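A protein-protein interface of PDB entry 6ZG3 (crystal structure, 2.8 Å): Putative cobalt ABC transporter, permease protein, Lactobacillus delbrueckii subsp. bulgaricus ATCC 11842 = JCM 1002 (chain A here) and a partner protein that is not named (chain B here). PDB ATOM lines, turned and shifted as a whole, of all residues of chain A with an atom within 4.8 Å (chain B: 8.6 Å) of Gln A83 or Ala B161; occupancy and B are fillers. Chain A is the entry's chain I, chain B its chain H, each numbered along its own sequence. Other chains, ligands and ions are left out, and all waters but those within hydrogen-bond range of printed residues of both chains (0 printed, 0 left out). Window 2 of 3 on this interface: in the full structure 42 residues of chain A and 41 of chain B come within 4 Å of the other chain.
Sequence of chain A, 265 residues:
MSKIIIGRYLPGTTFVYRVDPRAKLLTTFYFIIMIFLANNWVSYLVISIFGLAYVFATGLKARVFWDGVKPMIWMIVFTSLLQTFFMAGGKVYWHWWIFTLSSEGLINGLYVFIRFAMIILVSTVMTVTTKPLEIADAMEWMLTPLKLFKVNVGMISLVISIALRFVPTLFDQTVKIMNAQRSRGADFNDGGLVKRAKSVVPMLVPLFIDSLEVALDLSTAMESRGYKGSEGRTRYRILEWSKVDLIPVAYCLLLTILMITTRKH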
ATOM      1  N   THR A  79       2.458 -21.577  14.904  1.00  0.00           N
ATOM      2  CA  THR A  79       2.494 -20.714  13.727  1.00  0.00           C
ATOM      3  C   THR A  79       1.145 -20.625  13.027  1.00  0.00           C
ATOM      4  O   THR A  79       0.949 -19.731  12.202  1.00  0.00           O
ATOM      5  CB  THR A  79       3.561 -21.201  12.749  1.00  0.00           C
ATOM      6  OG1 THR A  79       3.489 -22.630  12.651  1.00  0.00           O
ATOM      7  CG2 THR A  79       4.951 -20.802  13.239  1.00  0.00           C
ATOM      8  N   SER A  80       0.257 -21.589  13.269  1.00  0.00           N
ATOM      9  CA  SER A  80      -1.090 -21.586  12.712  1.00  0.00           C
ATOM     10  C   SER A  80      -1.999 -20.631  13.448  1.00  0.00           C
ATOM     11  O   SER A  80      -2.682 -19.826  12.826  1.00  0.00           O
ATOM     12  CB  SER A  80      -1.692 -22.989  12.780  1.00  0.00           C
ATOM     13  OG  SER A  80      -0.958 -23.932  12.035  1.00  0.00           O
ATOM     14  N   LEU A  81      -2.053 -20.736  14.778  1.00  0.00           N
ATOM     15  CA  LEU A  81      -2.902 -19.834  15.553  1.00  0.00           C
ATOM     16  C   LEU A  81      -2.346 -18.409  15.559  1.00  0.00           C
ATOM     17  O   LEU A  81      -3.119 -17.447  15.529  1.00  0.00           O
ATOM     18  CB  LEU A  81      -3.120 -20.388  16.967  1.00  0.00           C
ATOM     19  CG  LEU A  81      -1.996 -20.487  18.010  1.00  0.00           C
ATOM     20  CD1 LEU A  81      -1.930 -19.222  18.873  1.00  0.00           C
ATOM     21  CD2 LEU A  81      -2.148 -21.750  18.865  1.00  0.00           C
ATOM     22  N   LEU A  82      -1.012 -18.240  15.607  1.00  0.00           N
ATOM     23  CA  LEU A  82      -0.438 -16.901  15.425  1.00  0.00           C
ATOM     24  C   LEU A  82      -0.868 -16.280  14.103  1.00  0.00           C
ATOM     25  O   LEU A  82      -1.004 -15.057  14.005  1.00  0.00           O
ATOM     26  CB  LEU A  82       1.095 -16.939  15.496  1.00  0.00           C
ATOM     27  CG  LEU A  82       1.775 -16.722  16.856  1.00  0.00           C
ATOM     28  CD1 LEU A  82       1.174 -17.631  17.926  1.00  0.00           C
ATOM     29  CD2 LEU A  82       3.292 -16.918  16.758  1.00  0.00           C
ATOM     30  N   GLN A  83      -1.043 -17.097  13.070  1.00  0.00           N
ATOM     31  CA  GLN A  83      -1.445 -16.587  11.766  1.00  0.00           C
ATOM     32  C   GLN A  83      -2.956 -16.383  11.683  1.00  0.00           C
ATOM     33  O   GLN A  83      -3.413 -15.347  11.197  1.00  0.00           O
ATOM     34  CB  GLN A  83      -0.946 -17.566  10.695  1.00  0.00           C
ATOM     35  CG  GLN A  83      -0.935 -17.169   9.199  1.00  0.00           C
ATOM     36  CD  GLN A  83      -1.476 -15.812   8.848  1.00  0.00           C
ATOM     37  OE1 GLN A  83      -2.684 -15.623   8.769  1.00  0.00           O
ATOM     38  NE2 GLN A  83      -0.584 -14.880   8.544  1.00  0.00           N
ATOM     39  N   THR A  84      -3.744 -17.333  12.200  1.00  0.00           N
ATOM     40  CA  THR A  84      -5.200 -17.227  12.132  1.00  0.00           C
ATOM     41  C   THR A  84      -5.674 -15.926  12.761  1.00  0.00           C
ATOM     42  O   THR A  84      -6.502 -15.209  12.188  1.00  0.00           O
ATOM     43  CB  THR A  84      -5.880 -18.428  12.809  1.00  0.00           C
ATOM     44  OG1 THR A  84      -5.423 -18.568  14.159  1.00  0.00           O
ATOM     45  CG2 THR A  84      -5.614 -19.715  12.041  1.00  0.00           C
ATOM     46  N   PHE A  85      -5.133 -15.589  13.931  1.00  0.00           N
ATOM     47  CA  PHE A  85      -5.538 -14.380  14.628  1.00  0.00           C
ATOM     48  C   PHE A  85      -4.978 -13.132  13.967  1.00  0.00           C
ATOM     49  O   PHE A  85      -5.430 -12.031  14.284  1.00  0.00           O
ATOM     50  CB  PHE A  85      -5.061 -14.425  16.077  1.00  0.00           C
ATOM     51  CG  PHE A  85      -5.727 -15.480  16.925  1.00  0.00           C
ATOM     52  CD1 PHE A  85      -7.049 -15.844  16.716  1.00  0.00           C
ATOM     53  CD2 PHE A  85      -5.020 -16.102  17.944  1.00  0.00           C
ATOM     54  CE1 PHE A  85      -7.649 -16.808  17.514  1.00  0.00           C
ATOM     55  CE2 PHE A  85      -5.609 -17.066  18.740  1.00  0.00           C
ATOM     56  CZ  PHE A  85      -6.928 -17.420  18.526  1.00  0.00           C
ATOM     57  N   PHE A  86      -4.037 -13.291  13.034  1.00  0.00           N
ATOM     58  CA  PHE A  86      -3.241 -12.222  12.425  1.00  0.00           C
ATOM     59  C   PHE A  86      -2.319 -11.543  13.430  1.00  0.00           C
ATOM     60  O   PHE A  86      -1.269 -12.087  13.787  1.00  0.00           O
ATOM     61  CB  PHE A  86      -4.134 -11.164  11.752  1.00  0.00           C
ATOM     62  CG  PHE A  86      -5.199 -11.745  10.866  1.00  0.00           C
ATOM     63  CD1 PHE A  86      -4.913 -12.087   9.543  1.00  0.00           C
ATOM     64  CD2 PHE A  86      -6.486 -11.939  11.346  1.00  0.00           C
ATOM     65  CE1 PHE A  86      -5.880 -12.624   8.716  1.00  0.00           C
ATOM     66  CE2 PHE A  86      -7.468 -12.474  10.532  1.00  0.00           C
ATOM     67  CZ  PHE A  86      -7.164 -12.817   9.207  1.00  0.00           C
ATOM     68  N   ASN A 108      -6.992 -19.000   6.280  1.00  0.00           N
ATOM     69  CA  ASN A 108      -5.624 -18.535   6.097  1.00  0.00           C
ATOM     70  C   ASN A 108      -4.640 -19.412   6.864  1.00  0.00           C
ATOM     71  O   ASN A 108      -3.608 -19.821   6.321  1.00  0.00           O
ATOM     72  CB  ASN A 108      -5.515 -17.076   6.540  1.00  0.00           C
ATOM     73  CG  ASN A 108      -5.952 -16.092   5.462  1.00  0.00           C
ATOM     74  OD1 ASN A 108      -7.106 -15.658   5.438  1.00  0.00           O
ATOM     75  ND2 ASN A 108      -5.032 -15.729   4.576  1.00  0.00           N
ATOM     76  N   GLY A 109      -4.938 -19.713   8.132  1.00  0.00           N
ATOM     77  CA  GLY A 109      -4.051 -20.594   8.878  1.00  0.00           C
ATOM     78  C   GLY A 109      -4.119 -22.036   8.425  1.00  0.00           C
ATOM     79  O   GLY A 109      -3.182 -22.811   8.675  1.00  0.00           O
ATOM     80  N   VAL A 112      -1.113 -22.251   6.307  1.00  0.00           N
ATOM     81  CA  VAL A 112       0.133 -22.587   6.986  1.00  0.00           C
ATOM     82  C   VAL A 112       0.189 -24.079   7.285  1.00  0.00           C
ATOM     83  O   VAL A 112       1.249 -24.709   7.143  1.00  0.00           O
ATOM     84  CB  VAL A 112       0.336 -21.726   8.251  1.00  0.00           C
ATOM     85  CG1 VAL A 112      -0.165 -20.313   8.016  1.00  0.00           C
ATOM     86  CG2 VAL A 112      -0.286 -22.356   9.471  1.00  0.00           C
ATOM     87  N   LEU B  85       9.726 -19.129  15.729  1.00  0.00           N
ATOM     88  CA  LEU B  85       9.190 -18.062  14.889  1.00  0.00           C
ATOM     89  C   LEU B  85      10.296 -17.167  14.335  1.00  0.00           C
ATOM     90  O   LEU B  85      10.104 -16.520  13.303  1.00  0.00           O
ATOM     91  CB  LEU B  85       8.190 -17.220  15.684  1.00  0.00           C
ATOM     92  CG  LEU B  85       7.403 -16.125  14.966  1.00  0.00           C
ATOM     93  CD1 LEU B  85       6.061 -16.694  14.551  1.00  0.00           C
ATOM     94  CD2 LEU B  85       7.232 -14.863  15.819  1.00  0.00           C
ATOM     95  N   PRO B 155       7.523  -3.850   6.265  1.00  0.00           N
ATOM     96  CA  PRO B 155       7.035  -4.933   7.130  1.00  0.00           C
ATOM     97  C   PRO B 155       6.123  -5.898   6.403  1.00  0.00           C
ATOM     98  O   PRO B 155       5.262  -6.521   7.022  1.00  0.00           O
ATOM     99  CB  PRO B 155       6.252  -4.182   8.212  1.00  0.00           C
ATOM    100  CG  PRO B 155       6.746  -2.781   8.130  1.00  0.00           C
ATOM    101  CD  PRO B 155       6.986  -2.553   6.680  1.00  0.00           C
ATOM    102  N   GLN B 156       6.321  -6.037   5.097  1.00  0.00           N
ATOM    103  CA  GLN B 156       5.635  -7.041   4.293  1.00  0.00           C
ATOM    104  C   GLN B 156       6.542  -8.267   4.231  1.00  0.00           C
ATOM    105  O   GLN B 156       7.216  -8.550   3.236  1.00  0.00           O
ATOM    106  CB  GLN B 156       5.297  -6.490   2.916  1.00  0.00           C
ATOM    107  CG  GLN B 156       4.167  -5.427   2.851  1.00  0.00           C
ATOM    108  CD  GLN B 156       4.333  -4.226   3.809  1.00  0.00           C
ATOM    109  OE1 GLN B 156       5.443  -3.722   4.028  1.00  0.00           O
ATOM    110  NE2 GLN B 156       3.209  -3.740   4.340  1.00  0.00           N
ATOM    111  N   LYS B 157       6.601  -8.942   5.378  1.00  0.00           N
ATOM    112  CA  LYS B 157       7.434 -10.109   5.606  1.00  0.00           C
ATOM    113  C   LYS B 157       6.853 -11.395   5.062  1.00  0.00           C
ATOM    114  O   LYS B 157       7.583 -12.388   4.961  1.00  0.00           O
ATOM    115  CB  LYS B 157       7.683 -10.285   7.103  1.00  0.00           C
ATOM    116  CG  LYS B 157       6.513  -9.862   7.982  1.00  0.00           C
ATOM    117  CD  LYS B 157       6.980  -9.292   9.324  1.00  0.00           C
ATOM    118  CE  LYS B 157       8.040  -8.212   9.150  1.00  0.00           C
ATOM    119  NZ  LYS B 157       9.424  -8.773   9.096  1.00  0.00           N
ATOM    120  N   LEU B 158       5.555 -11.421   4.766  1.00  0.00           N
ATOM    121  CA  LEU B 158       4.826 -12.648   4.456  1.00  0.00           C
ATOM    122  C   LEU B 158       4.899 -13.626   5.627  1.00  0.00           C
ATOM    123  O   LEU B 158       4.351 -14.731   5.564  1.00  0.00           O
ATOM    124  CB  LEU B 158       5.304 -13.300   3.151  1.00  0.00           C
ATOM    125  CG  LEU B 158       4.656 -12.674   1.904  1.00  0.00           C
ATOM    126  CD1 LEU B 158       4.859 -13.557   0.681  1.00  0.00           C
ATOM    127  CD2 LEU B 158       3.175 -12.377   2.125  1.00  0.00           C
ATOM    128  N   ALA B 159       5.623 -13.250   6.678  1.00  0.00           N
ATOM    129  CA  ALA B 159       5.541 -13.976   7.933  1.00  0.00           C
ATOM    130  C   ALA B 159       4.093 -14.089   8.369  1.00  0.00           C
ATOM    131  O   ALA B 159       3.598 -15.182   8.654  1.00  0.00           O
ATOM    132  CB  ALA B 159       6.360 -13.247   8.982  1.00  0.00           C
ATOM    133  N   LEU B 160       3.407 -12.955   8.430  1.00  0.00           N
ATOM    134  CA  LEU B 160       2.002 -12.875   8.776  1.00  0.00           C
ATOM    135  C   LEU B 160       1.439 -11.670   8.045  1.00  0.00           C
ATOM    136  O   LEU B 160       2.142 -10.984   7.300  1.00  0.00           O
ATOM    137  CB  LEU B 160       1.762 -12.705  10.278  1.00  0.00           C
ATOM    138  CG  LEU B 160       2.082 -13.785  11.319  1.00  0.00           C
ATOM    139  CD1 LEU B 160       1.521 -13.390  12.688  1.00  0.00           C
ATOM    140  CD2 LEU B 160       1.622 -15.169  10.929  1.00  0.00           C
ATOM    141  N   ALA B 161       0.157 -11.420   8.267  1.00  0.00           N
ATOM    142  CA  ALA B 161      -0.482 -10.203   7.786  1.00  0.00           C
ATOM    143  C   ALA B 161      -0.502  -9.179   8.905  1.00  0.00           C
ATOM    144  O   ALA B 161      -1.492  -8.466   9.112  1.00  0.00           O
ATOM    145  CB  ALA B 161      -1.891 -10.491   7.272  1.00  0.00           C
ATOM    146  N   LEU B 162       0.618  -9.066   9.618  1.00  0.00           N
ATOM    147  CA  LEU B 162       0.666  -8.193  10.780  1.00  0.00           C
ATOM    148  C   LEU B 162       0.725  -6.738  10.346  1.00  0.00           C
ATOM    149  O   LEU B 162       1.474  -6.374   9.437  1.00  0.00           O
ATOM    150  CB  LEU B 162       1.899  -8.521  11.623  1.00  0.00           C
ATOM    151  CG  LEU B 162       1.900  -9.695  12.592  1.00  0.00           C
ATOM    152  CD1 LEU B 162       3.274 -10.344  12.634  1.00  0.00           C
ATOM    153  CD2 LEU B 162       1.542  -9.184  13.958  1.00  0.00           C
ATOM    154  N   GLY B 163      -0.062  -5.904  11.022  1.00  0.00           N
ATOM    155  CA  GLY B 163      -0.114  -4.493  10.703  1.00  0.00           C
ATOM    156  C   GLY B 163       1.268  -3.886  10.670  1.00  0.00           C
ATOM    157  O   GLY B 163       2.106  -4.240  11.503  1.00  0.00           O
ATOM    158  N   ALA B 164       1.533  -3.015   9.693  1.00  0.00           N
ATOM    159  CA  ALA B 164       2.884  -2.501   9.530  1.00  0.00           C
ATOM    160  C   ALA B 164       3.388  -1.940  10.847  1.00  0.00           C
ATOM    161  O   ALA B 164       4.542  -2.160  11.229  1.00  0.00           O
ATOM    162  CB  ALA B 164       2.918  -1.442   8.436  1.00  0.00           C
ATOM    163  N   SER B 166       2.186  -2.938  13.839  1.00  0.00           N
ATOM    164  CA  SER B 166       2.345  -4.140  14.659  1.00  0.00           C
ATOM    165  C   SER B 166       3.543  -4.956  14.196  1.00  0.00           C
ATOM    166  O   SER B 166       4.275  -5.523  15.016  1.00  0.00           O
ATOM    167  CB  SER B 166       1.072  -4.998  14.631  1.00  0.00           C
ATOM    168  OG  SER B 166       0.026  -4.453  15.426  1.00  0.00           O
ATOM    169  N   GLY B 167       3.761  -5.026  12.883  1.00  0.00           N
ATOM    170  CA  GLY B 167       4.949  -5.691  12.385  1.00  0.00           C
ATOM    171  C   GLY B 167       6.221  -5.057  12.915  1.00  0.00           C
ATOM    172  O   GLY B 167       7.156  -5.754  13.308  1.00  0.00           O
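CD1 of Leu B85 touches CD2 of Leu A82 (3.5 Å).
Leu A82 touches Leu B160 (O to CD1, 3.3 Å).
Leu B160 touches Gln A83.
Ala B161 touches Gln A83 (N to NE2, 3.5 Å).
Leu B160 touches Phe A86.
Of chain B, only Leu B160 (3.3 Å) and Ala B161 (3.5 Å) come within 4 Å of Gln A83.
Ala B161 touches just one residue of chain A: Gln A83 (3.5 Å).
Printed residues of chain A within 4 Å of Leu B160: Leu A82 (3.3 Å), Gln A83 (3.3 Å) and Phe A86 (3.3 Å).
Printed residues of chain B within 4 Å of Phe A86: Leu B160.
Of the printed residues of chain B, Leu A82 touches Leu B85 and Leu B160.
Of the printed residues of chain A, Leu B85 touches Leu A82 (3.5 Å).
The nearest residue of chain B that does not touch Gln A83 is Ala B159 (4.2 Å).
Of the 11 printed residues of chain A, 3 touch a printed residue of chain B.
Printed residues of chain A that touch a printed residue of chain B: Leu A82, Gln A83 and Phe A86.
Hydrophobic or aromatic side chains of chain A within 4 Å of the printed part of chain B: Leu A82.
Of the 13 printed residues of chain B, 3 touch a printed residue of chain A.
Printed residues of chain B that touch a printed residue of chain A: Leu B85, Leu B160 and Ala B161.
Hydrophobic or aromatic side chains of chain B within 4 Å of the printed part of chain A: Leu B85 and Leu B160.
Among the printed residues, 5 pairs touch across the chains.
Among the printed residues, no Asp or Glu carboxylate lies within 4 Å of a Lys or Arg side-chain nitrogen of the other chain.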
